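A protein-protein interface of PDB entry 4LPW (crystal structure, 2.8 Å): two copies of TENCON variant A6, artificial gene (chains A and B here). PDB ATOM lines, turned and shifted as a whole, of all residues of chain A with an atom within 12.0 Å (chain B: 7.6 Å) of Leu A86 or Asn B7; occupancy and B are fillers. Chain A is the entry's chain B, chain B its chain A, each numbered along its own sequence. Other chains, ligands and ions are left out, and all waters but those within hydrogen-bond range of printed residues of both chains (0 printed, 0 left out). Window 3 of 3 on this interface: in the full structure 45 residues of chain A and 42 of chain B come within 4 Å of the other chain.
Printed residues of chain B within 4 Å of Asn A84: Ala B4.
Of the printed residues of chain B, Pro A85 touches Ile B72 and Tyr B73.
Leu A86 touches seven residues of chain B.
Printed residues of chain B within 4 Å of Ala A88: Leu B8 (3.8 Å) and Val B70 (2.8 Å).
Glu A89 touches none of the printed residues of chain B.
Of the printed residues of chain A, Ala B4 touches Ser A83 and Asn A84.
Of chain A, only Ser A83 and Leu A86 come within 4 Å of Pro B5.
Asn B7 touches just one residue of chain A: Leu A86.
Printed residues of chain A within 4 Å of Leu B8: Leu A86 (3.6 Å), Ala A88 (3.8 Å) and Phe A90 (3.96 Å).
No residue of chain A comes within 4 Å of Thr B23.
Printed residues of chain A within 4 Å of Leu B33: Met A82 (3.6 Å).
Val B70 touches just these residues of chain A: Leu A86 (3.7 Å), Ser A87 (3.1 Å) and Ala A88 (2.8 Å).
Ser B71 touches just these residues of chain A: Leu A86 and Ser A87.
Ile B72 touches just these residues of chain A: Pro A85 and Leu A86.
Of the printed residues of chain A, Tyr B73 touches Met A82 (3.7 Å), Ser A83 (3.8 Å) and Pro A85 (3.5 Å).
The nearest residue of chain B that does not touch Leu A86 is Trp B22 (4.9 Å).
O of Val B70 is in hydrogen-bond range of N of Ala A88 (2.8 Å).
The side-chain hydroxyl (OG) of Ser B71 lies within hydrogen-bond range of the side-chain hydroxyl (OG) of Ser A87 (2.9 Å).
N of Ile B72 is in hydrogen-bond range of O of Leu A86 (2.8 Å).
The backbone carbonyl oxygen (O) of Gly B74 is in hydrogen-bond range of the backbone NH (N) of Ser A83, 2.9 Å away.
Printed residues of chain A that touch a printed residue of chain B: Met A82, Ser A83, Asn A84, Pro A85, Leu A86, Ser A87, Ala A88 and Phe A90.
Hydrophobic or aromatic side chains of chain A within 4 Å of the printed part of chain B: Met A82, Pro A85, Leu A86, Ala A88 and Phe A90.
Of the 19 printed residues of chain B, 12 touch a printed residue of chain A.
Hydrophobic or aromatic side chains of chain B that line the printed part of chain A: Ala B4, Pro B5, Leu B8, Val B10, Leu B33, Val B70, Ile B72 and Tyr B73.
Among the printed residues, 23 pairs touch across the chains.
No position is printed for both chains.
Of the 23 pairs that touch across the chains among the printed residues, none has its exchanged pair printed and touching as well.
Among the printed residues, pairs that only touch across the chains: Met A82 with Gly B74, Leu A86 with Ser B71, Ser A87 with Val B70, Ser A83 with Pro B5, Leu A86 with Lys B6, Pro A85 with Tyr B73, Leu A86 with Leu B8, Met A82 with Leu B33, Pro A85 with Ile B72, Met A82 with Tyr B73, Leu A86 with Val B70, Leu A86 with Asn B7, Leu A86 with Pro B5, Ser A83 with Ala B4, Ser A83 with Tyr B73, Ala A88 with Leu B8, Phe A90 with Val B10, Asn A84 with Ala B4 and Phe A90 with Leu B8.
The backbone NH of Lys B6 lies within hydrogen-bond range of the backbone carbonyl oxygen of Thr B23, at 2.6 Å.
N of Tyr B73 is in hydrogen-bond range of O of Leu B33, 2.8 Å away.
N of Gln B35 lies within hydrogen-bond range of O of Ser B71.
The side-chain hydroxyl of Tyr B73 lies within hydrogen-bond range of the side-chain amide oxygen of Gln B35, at 2.9 Å.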
ATOM      1  N   MET A  82     -23.342 -15.447   7.042  1.00  0.00           N
ATOM      2  CA  MET A  82     -22.983 -16.366   5.965  1.00  0.00           C
ATOM      3  C   MET A  82     -24.198 -17.017   5.305  1.00  0.00           C
ATOM      4  O   MET A  82     -25.301 -17.009   5.860  1.00  0.00           O
ATOM      5  CB  MET A  82     -21.897 -17.390   6.372  1.00  0.00           C
ATOM      6  CG  MET A  82     -22.148 -18.155   7.666  1.00  0.00           C
ATOM      7  SD  MET A  82     -20.739 -19.201   8.159  1.00  0.00           S
ATOM      8  CE  MET A  82     -19.340 -18.107   7.814  1.00  0.00           C
ATOM      9  N   SER A  83     -23.985 -17.535   4.098  1.00  0.00           N
ATOM     10  CA  SER A  83     -25.012 -18.234   3.354  1.00  0.00           C
ATOM     11  C   SER A  83     -25.088 -19.659   3.851  1.00  0.00           C
ATOM     12  O   SER A  83     -24.282 -20.087   4.661  1.00  0.00           O
ATOM     13  CB  SER A  83     -24.665 -18.234   1.874  1.00  0.00           C
ATOM     14  OG  SER A  83     -23.409 -18.856   1.674  1.00  0.00           O
ATOM     15  N   ASN A  84     -26.076 -20.396   3.372  1.00  0.00           N
ATOM     16  CA  ASN A  84     -26.150 -21.809   3.690  1.00  0.00           C
ATOM     17  C   ASN A  84     -25.029 -22.538   2.966  1.00  0.00           C
ATOM     18  O   ASN A  84     -24.710 -22.229   1.806  1.00  0.00           O
ATOM     19  CB  ASN A  84     -27.524 -22.380   3.355  1.00  0.00           C
ATOM     20  CG  ASN A  84     -28.574 -21.967   4.366  1.00  0.00           C
ATOM     21  OD1 ASN A  84     -28.279 -21.849   5.566  1.00  0.00           O
ATOM     22  ND2 ASN A  84     -29.800 -21.713   3.891  1.00  0.00           N
ATOM     23  N   PRO A  85     -24.405 -23.494   3.659  1.00  0.00           N
ATOM     24  CA  PRO A  85     -23.226 -24.161   3.126  1.00  0.00           C
ATOM     25  C   PRO A  85     -23.526 -24.926   1.847  1.00  0.00           C
ATOM     26  O   PRO A  85     -24.626 -25.450   1.650  1.00  0.00           O
ATOM     27  CB  PRO A  85     -22.849 -25.133   4.242  1.00  0.00           C
ATOM     28  CG  PRO A  85     -24.098 -25.381   4.954  1.00  0.00           C
ATOM     29  CD  PRO A  85     -24.862 -24.108   4.913  1.00  0.00           C
ATOM     30  N   LEU A  86     -22.540 -24.969   0.967  1.00  0.00           N
ATOM     31  CA  LEU A  86     -22.610 -25.833  -0.187  1.00  0.00           C
ATOM     32  C   LEU A  86     -21.717 -27.015   0.148  1.00  0.00           C
ATOM     33  O   LEU A  86     -20.491 -26.883   0.222  1.00  0.00           O
ATOM     34  CB  LEU A  86     -22.094 -25.091  -1.419  1.00  0.00           C
ATOM     35  CG  LEU A  86     -22.250 -25.668  -2.826  1.00  0.00           C
ATOM     36  CD1 LEU A  86     -23.717 -25.947  -3.158  1.00  0.00           C
ATOM     37  CD2 LEU A  86     -21.658 -24.674  -3.809  1.00  0.00           C
ATOM     38  N   SER A  87     -22.330 -28.167   0.372  1.00  0.00           N
ATOM     39  CA  SER A  87     -21.561 -29.333   0.776  1.00  0.00           C
ATOM     40  C   SER A  87     -21.428 -30.342  -0.359  1.00  0.00           C
ATOM     41  O   SER A  87     -22.228 -30.323  -1.303  1.00  0.00           O
ATOM     42  CB  SER A  87     -22.198 -29.987   2.004  1.00  0.00           C
ATOM     43  OG  SER A  87     -22.289 -29.058   3.077  1.00  0.00           O
ATOM     44  N   ALA A  88     -20.416 -31.207  -0.260  1.00  0.00           N
ATOM     45  CA  ALA A  88     -20.200 -32.285  -1.219  1.00  0.00           C
ATOM     46  C   ALA A  88     -19.202 -33.262  -0.652  1.00  0.00           C
ATOM     47  O   ALA A  88     -18.461 -32.913   0.245  1.00  0.00           O
ATOM     48  CB  ALA A  88     -19.710 -31.730  -2.550  1.00  0.00           C
ATOM     49  N   GLU A  89     -19.200 -34.486  -1.172  1.00  0.00           N
ATOM     50  CA  GLU A  89     -18.257 -35.514  -0.745  1.00  0.00           C
ATOM     51  C   GLU A  89     -17.304 -35.837  -1.878  1.00  0.00           C
ATOM     52  O   GLU A  89     -17.710 -36.391  -2.909  1.00  0.00           O
ATOM     53  CB  GLU A  89     -18.972 -36.807  -0.368  1.00  0.00           C
ATOM     54  CG  GLU A  89     -19.950 -36.728   0.768  1.00  0.00           C
ATOM     55  CD  GLU A  89     -20.870 -37.946   0.801  1.00  0.00           C
ATOM     56  OE1 GLU A  89     -21.633 -38.151  -0.174  1.00  0.00           O
ATOM     57  OE2 GLU A  89     -20.806 -38.719   1.784  1.00  0.00           O
ATOM     58  N   PHE A  90     -16.032 -35.512  -1.682  1.00  0.00           N
ATOM     59  CA  PHE A  90     -15.020 -35.778  -2.689  1.00  0.00           C
ATOM     60  C   PHE A  90     -13.953 -36.699  -2.118  1.00  0.00           C
ATOM     61  O   PHE A  90     -13.643 -36.623  -0.934  1.00  0.00           O
ATOM     62  CB  PHE A  90     -14.425 -34.463  -3.191  1.00  0.00           C
ATOM     63  CG  PHE A  90     -15.430 -33.560  -3.857  1.00  0.00           C
ATOM     64  CD1 PHE A  90     -16.405 -34.084  -4.683  1.00  0.00           C
ATOM     65  CD2 PHE A  90     -15.411 -32.194  -3.643  1.00  0.00           C
ATOM     66  CE1 PHE A  90     -17.318 -33.267  -5.295  1.00  0.00           C
ATOM     67  CE2 PHE A  90     -16.334 -31.369  -4.259  1.00  0.00           C
ATOM     68  CZ  PHE A  90     -17.282 -31.913  -5.087  1.00  0.00           C
ATOM     69  N   ALA B   4     -26.460 -17.953  -2.109  1.00  0.00           N
ATOM     70  CA  ALA B   4     -25.291 -18.767  -1.782  1.00  0.00           C
ATOM     71  C   ALA B   4     -24.238 -18.876  -2.898  1.00  0.00           C
ATOM     72  O   ALA B   4     -24.424 -18.339  -3.976  1.00  0.00           O
ATOM     73  CB  ALA B   4     -25.760 -20.163  -1.335  1.00  0.00           C
ATOM     74  N   PRO B   5     -23.107 -19.555  -2.621  1.00  0.00           N
ATOM     75  CA  PRO B   5     -22.268 -20.034  -3.717  1.00  0.00           C
ATOM     76  C   PRO B   5     -22.998 -21.147  -4.440  1.00  0.00           C
ATOM     77  O   PRO B   5     -23.939 -21.712  -3.868  1.00  0.00           O
ATOM     78  CB  PRO B   5     -21.065 -20.634  -2.996  1.00  0.00           C
ATOM     79  CG  PRO B   5     -21.012 -19.974  -1.705  1.00  0.00           C
ATOM     80  CD  PRO B   5     -22.429 -19.705  -1.321  1.00  0.00           C
ATOM     81  N   LYS B   6     -22.567 -21.482  -5.658  1.00  0.00           N
ATOM     82  CA  LYS B   6     -23.242 -22.513  -6.442  1.00  0.00           C
ATOM     83  C   LYS B   6     -22.293 -23.548  -7.004  1.00  0.00           C
ATOM     84  O   LYS B   6     -21.094 -23.292  -7.149  1.00  0.00           O
ATOM     85  CB  LYS B   6     -23.984 -21.887  -7.623  1.00  0.00           C
ATOM     86  CG  LYS B   6     -25.206 -21.064  -7.280  1.00  0.00           C
ATOM     87  CD  LYS B   6     -25.803 -20.522  -8.573  1.00  0.00           C
ATOM     88  CE  LYS B   6     -24.731 -19.848  -9.428  1.00  0.00           C
ATOM     89  NZ  LYS B   6     -25.258 -19.391 -10.746  1.00  0.00           N
ATOM     90  N   ASN B   7     -22.866 -24.703  -7.341  1.00  0.00           N
ATOM     91  CA  ASN B   7     -22.206 -25.721  -8.156  1.00  0.00           C
ATOM     92  C   ASN B   7     -20.728 -26.001  -7.814  1.00  0.00           C
ATOM     93  O   ASN B   7     -19.833 -25.746  -8.623  1.00  0.00           O
ATOM     94  CB  ASN B   7     -22.364 -25.382  -9.647  1.00  0.00           C
ATOM     95  CG  ASN B   7     -23.832 -25.286 -10.083  1.00  0.00           C
ATOM     96  OD1 ASN B   7     -24.696 -26.019  -9.600  1.00  0.00           O
ATOM     97  ND2 ASN B   7     -24.114 -24.364 -10.992  1.00  0.00           N
ATOM     98  N   LEU B   8     -20.493 -26.527  -6.612  1.00  0.00           N
ATOM     99  CA  LEU B   8     -19.163 -26.952  -6.163  1.00  0.00           C
ATOM    100  C   LEU B   8     -18.709 -28.169  -6.964  1.00  0.00           C
ATOM    101  O   LEU B   8     -19.412 -29.190  -7.021  1.00  0.00           O
ATOM    102  CB  LEU B   8     -19.192 -27.301  -4.658  1.00  0.00           C
ATOM    103  CG  LEU B   8     -17.950 -27.774  -3.871  1.00  0.00           C
ATOM    104  CD1 LEU B   8     -16.885 -26.692  -3.794  1.00  0.00           C
ATOM    105  CD2 LEU B   8     -18.295 -28.228  -2.461  1.00  0.00           C
ATOM    106  N   VAL B   9     -17.539 -28.069  -7.590  1.00  0.00           N
ATOM    107  CA  VAL B   9     -16.995 -29.202  -8.321  1.00  0.00           C
ATOM    108  C   VAL B   9     -15.569 -29.471  -7.902  1.00  0.00           C
ATOM    109  O   VAL B   9     -15.004 -28.744  -7.087  1.00  0.00           O
ATOM    110  CB  VAL B   9     -17.027 -28.981  -9.839  1.00  0.00           C
ATOM    111  CG1 VAL B   9     -18.476 -28.897 -10.346  1.00  0.00           C
ATOM    112  CG2 VAL B   9     -16.235 -27.733 -10.208  1.00  0.00           C
ATOM    113  N   VAL B  10     -14.981 -30.516  -8.471  1.00  0.00           N
ATOM    114  CA  VAL B  10     -13.646 -30.927  -8.078  1.00  0.00           C
ATOM    115  C   VAL B  10     -12.826 -31.313  -9.311  1.00  0.00           C
ATOM    116  O   VAL B  10     -13.361 -31.871 -10.274  1.00  0.00           O
ATOM    117  CB  VAL B  10     -13.720 -32.101  -7.076  1.00  0.00           C
ATOM    118  CG1 VAL B  10     -14.210 -33.363  -7.773  1.00  0.00           C
ATOM    119  CG2 VAL B  10     -12.368 -32.351  -6.420  1.00  0.00           C
ATOM    120  N   SER B  21     -13.583 -26.072  -7.058  1.00  0.00           N
ATOM    121  CA  SER B  21     -14.000 -24.955  -7.883  1.00  0.00           C
ATOM    122  C   SER B  21     -15.481 -24.709  -7.653  1.00  0.00           C
ATOM    123  O   SER B  21     -16.257 -25.652  -7.527  1.00  0.00           O
ATOM    124  CB  SER B  21     -13.729 -25.249  -9.354  1.00  0.00           C
ATOM    125  OG  SER B  21     -12.381 -25.637  -9.551  1.00  0.00           O
ATOM    126  N   TRP B  22     -15.865 -23.442  -7.576  1.00  0.00           N
ATOM    127  CA  TRP B  22     -17.254 -23.080  -7.347  1.00  0.00           C
ATOM    128  C   TRP B  22     -17.599 -21.800  -8.088  1.00  0.00           C
ATOM    129  O   TRP B  22     -16.726 -21.156  -8.684  1.00  0.00           O
ATOM    130  CB  TRP B  22     -17.532 -22.905  -5.854  1.00  0.00           C
ATOM    131  CG  TRP B  22     -16.726 -21.835  -5.226  1.00  0.00           C
ATOM    132  CD1 TRP B  22     -17.087 -20.533  -5.051  1.00  0.00           C
ATOM    133  CD2 TRP B  22     -15.397 -21.957  -4.683  1.00  0.00           C
ATOM    134  NE1 TRP B  22     -16.073 -19.842  -4.432  1.00  0.00           N
ATOM    135  CE2 TRP B  22     -15.035 -20.690  -4.204  1.00  0.00           C
ATOM    136  CE3 TRP B  22     -14.499 -23.019  -4.576  1.00  0.00           C
ATOM    137  CZ2 TRP B  22     -13.793 -20.457  -3.610  1.00  0.00           C
ATOM    138  CZ3 TRP B  22     -13.270 -22.780  -3.985  1.00  0.00           C
ATOM    139  CH2 TRP B  22     -12.930 -21.509  -3.508  1.00  0.00           C
ATOM    140  N   THR B  23     -18.881 -21.447  -8.046  1.00  0.00           N
ATOM    141  CA  THR B  23     -19.391 -20.208  -8.625  1.00  0.00           C
ATOM    142  C   THR B  23     -20.063 -19.367  -7.540  1.00  0.00           C
ATOM    143  O   THR B  23     -20.927 -19.857  -6.818  1.00  0.00           O
ATOM    144  CB  THR B  23     -20.459 -20.497  -9.710  1.00  0.00           C
ATOM    145  OG1 THR B  23     -19.923 -21.373 -10.715  1.00  0.00           O
ATOM    146  CG2 THR B  23     -20.940 -19.206 -10.351  1.00  0.00           C
ATOM    147  N   ALA B  24     -19.672 -18.105  -7.424  1.00  0.00           N
ATOM    148  CA  ALA B  24     -20.419 -17.169  -6.594  1.00  0.00           C
ATOM    149  C   ALA B  24     -20.800 -15.926  -7.394  1.00  0.00           C
ATOM    150  O   ALA B  24     -20.124 -15.578  -8.362  1.00  0.00           O
ATOM    151  CB  ALA B  24     -19.613 -16.781  -5.369  1.00  0.00           C
ATOM    152  N   LEU B  33     -15.584 -19.211   3.437  1.00  0.00           N
ATOM    153  CA  LEU B  33     -15.203 -20.154   4.465  1.00  0.00           C
ATOM    154  C   LEU B  33     -15.260 -21.555   3.879  1.00  0.00           C
ATOM    155  O   LEU B  33     -16.283 -21.982   3.327  1.00  0.00           O
ATOM    156  CB  LEU B  33     -16.110 -20.037   5.693  1.00  0.00           C
ATOM    157  CG  LEU B  33     -15.992 -21.112   6.785  1.00  0.00           C
ATOM    158  CD1 LEU B  33     -14.639 -21.100   7.457  1.00  0.00           C
ATOM    159  CD2 LEU B  33     -17.088 -20.906   7.815  1.00  0.00           C
ATOM    160  N   GLN B  35     -14.695 -25.592   4.844  1.00  0.00           N
ATOM    161  CA  GLN B  35     -14.594 -26.600   5.893  1.00  0.00           C
ATOM    162  C   GLN B  35     -14.407 -27.960   5.254  1.00  0.00           C
ATOM    163  O   GLN B  35     -15.101 -28.277   4.294  1.00  0.00           O
ATOM    164  CB  GLN B  35     -15.877 -26.621   6.731  1.00  0.00           C
ATOM    165  CG  GLN B  35     -15.850 -25.728   7.939  1.00  0.00           C
ATOM    166  CD  GLN B  35     -17.059 -25.936   8.829  1.00  0.00           C
ATOM    167  OE1 GLN B  35     -18.096 -26.432   8.373  1.00  0.00           O
ATOM    168  NE2 GLN B  35     -16.932 -25.567  10.108  1.00  0.00           N
ATOM    169  N   ARG B  55     -12.481 -18.420  -6.850  1.00  0.00           N
ATOM    170  CA  ARG B  55     -13.533 -19.327  -7.285  1.00  0.00           C
ATOM    171  C   ARG B  55     -12.972 -20.739  -7.343  1.00  0.00           C
ATOM    172  O   ARG B  55     -13.633 -21.670  -7.820  1.00  0.00           O
ATOM    173  CB  ARG B  55     -14.073 -18.915  -8.653  1.00  0.00           C
ATOM    174  CG  ARG B  55     -14.797 -17.581  -8.677  1.00  0.00           C
ATOM    175  CD  ARG B  55     -16.121 -17.666  -7.962  1.00  0.00           C
ATOM    176  NE  ARG B  55     -16.841 -16.392  -7.950  1.00  0.00           N
ATOM    177  CZ  ARG B  55     -16.578 -15.392  -7.116  1.00  0.00           C
ATOM    178  NH1 ARG B  55     -15.597 -15.505  -6.234  1.00  0.00           N
ATOM    179  NH2 ARG B  55     -17.287 -14.278  -7.169  1.00  0.00           N
ATOM    180  N   VAL B  70     -16.837 -31.843   2.301  1.00  0.00           N
ATOM    181  CA  VAL B  70     -16.354 -30.500   2.062  1.00  0.00           C
ATOM    182  C   VAL B  70     -17.544 -29.557   1.950  1.00  0.00           C
ATOM    183  O   VAL B  70     -18.488 -29.820   1.195  1.00  0.00           O
ATOM    184  CB  VAL B  70     -15.539 -30.450   0.748  1.00  0.00           C
ATOM    185  CG1 VAL B  70     -15.160 -29.017   0.391  1.00  0.00           C
ATOM    186  CG2 VAL B  70     -14.305 -31.322   0.871  1.00  0.00           C
ATOM    187  N   SER B  71     -17.499 -28.453   2.689  1.00  0.00           N
ATOM    188  CA  SER B  71     -18.557 -27.467   2.603  1.00  0.00           C
ATOM    189  C   SER B  71     -17.971 -26.084   2.455  1.00  0.00           C
ATOM    190  O   SER B  71     -17.006 -25.738   3.119  1.00  0.00           O
ATOM    191  CB  SER B  71     -19.439 -27.529   3.840  1.00  0.00           C
ATOM    192  OG  SER B  71     -19.643 -28.873   4.240  1.00  0.00           O
ATOM    193  N   ILE B  72     -18.560 -25.289   1.573  1.00  0.00           N
ATOM    194  CA  ILE B  72     -18.128 -23.907   1.422  1.00  0.00           C
ATOM    195  C   ILE B  72     -19.239 -22.889   1.702  1.00  0.00           C
ATOM    196  O   ILE B  72     -20.358 -22.991   1.190  1.00  0.00           O
ATOM    197  CB  ILE B  72     -17.497 -23.640   0.052  1.00  0.00           C
ATOM    198  CG1 ILE B  72     -17.175 -22.160  -0.074  1.00  0.00           C
ATOM    199  CG2 ILE B  72     -18.430 -24.051  -1.044  1.00  0.00           C
ATOM    200  CD1 ILE B  72     -15.948 -21.887  -0.873  1.00  0.00           C
ATOM    201  N   TYR B  73     -18.920 -21.899   2.523  1.00  0.00           N
ATOM    202  CA  TYR B  73     -19.881 -20.860   2.825  1.00  0.00           C
ATOM    203  C   TYR B  73     -19.465 -19.581   2.123  1.00  0.00           C
ATOM    204  O   TYR B  73     -18.277 -19.363   1.854  1.00  0.00           O
ATOM    205  CB  TYR B  73     -19.933 -20.584   4.319  1.00  0.00           C
ATOM    206  CG  TYR B  73     -20.091 -21.786   5.200  1.00  0.00           C
ATOM    207  CD1 TYR B  73     -19.037 -22.652   5.432  1.00  0.00           C
ATOM    208  CD2 TYR B  73     -21.285 -22.020   5.854  1.00  0.00           C
ATOM    209  CE1 TYR B  73     -19.185 -23.740   6.254  1.00  0.00           C
ATOM    210  CE2 TYR B  73     -21.441 -23.100   6.691  1.00  0.00           C
ATOM    211  CZ  TYR B  73     -20.392 -23.954   6.886  1.00  0.00           C
ATOM    212  OH  TYR B  73     -20.566 -25.025   7.724  1.00  0.00           O
ATOM    213  N   GLY B  74     -20.452 -18.735   1.842  1.00  0.00           N
ATOM    214  CA  GLY B  74     -20.194 -17.374   1.422  1.00  0.00           C
ATOM    215  C   GLY B  74     -20.350 -16.472   2.643  1.00  0.00           C
ATOM    216  O   GLY B  74     -21.350 -16.554   3.354  1.00  0.00           O
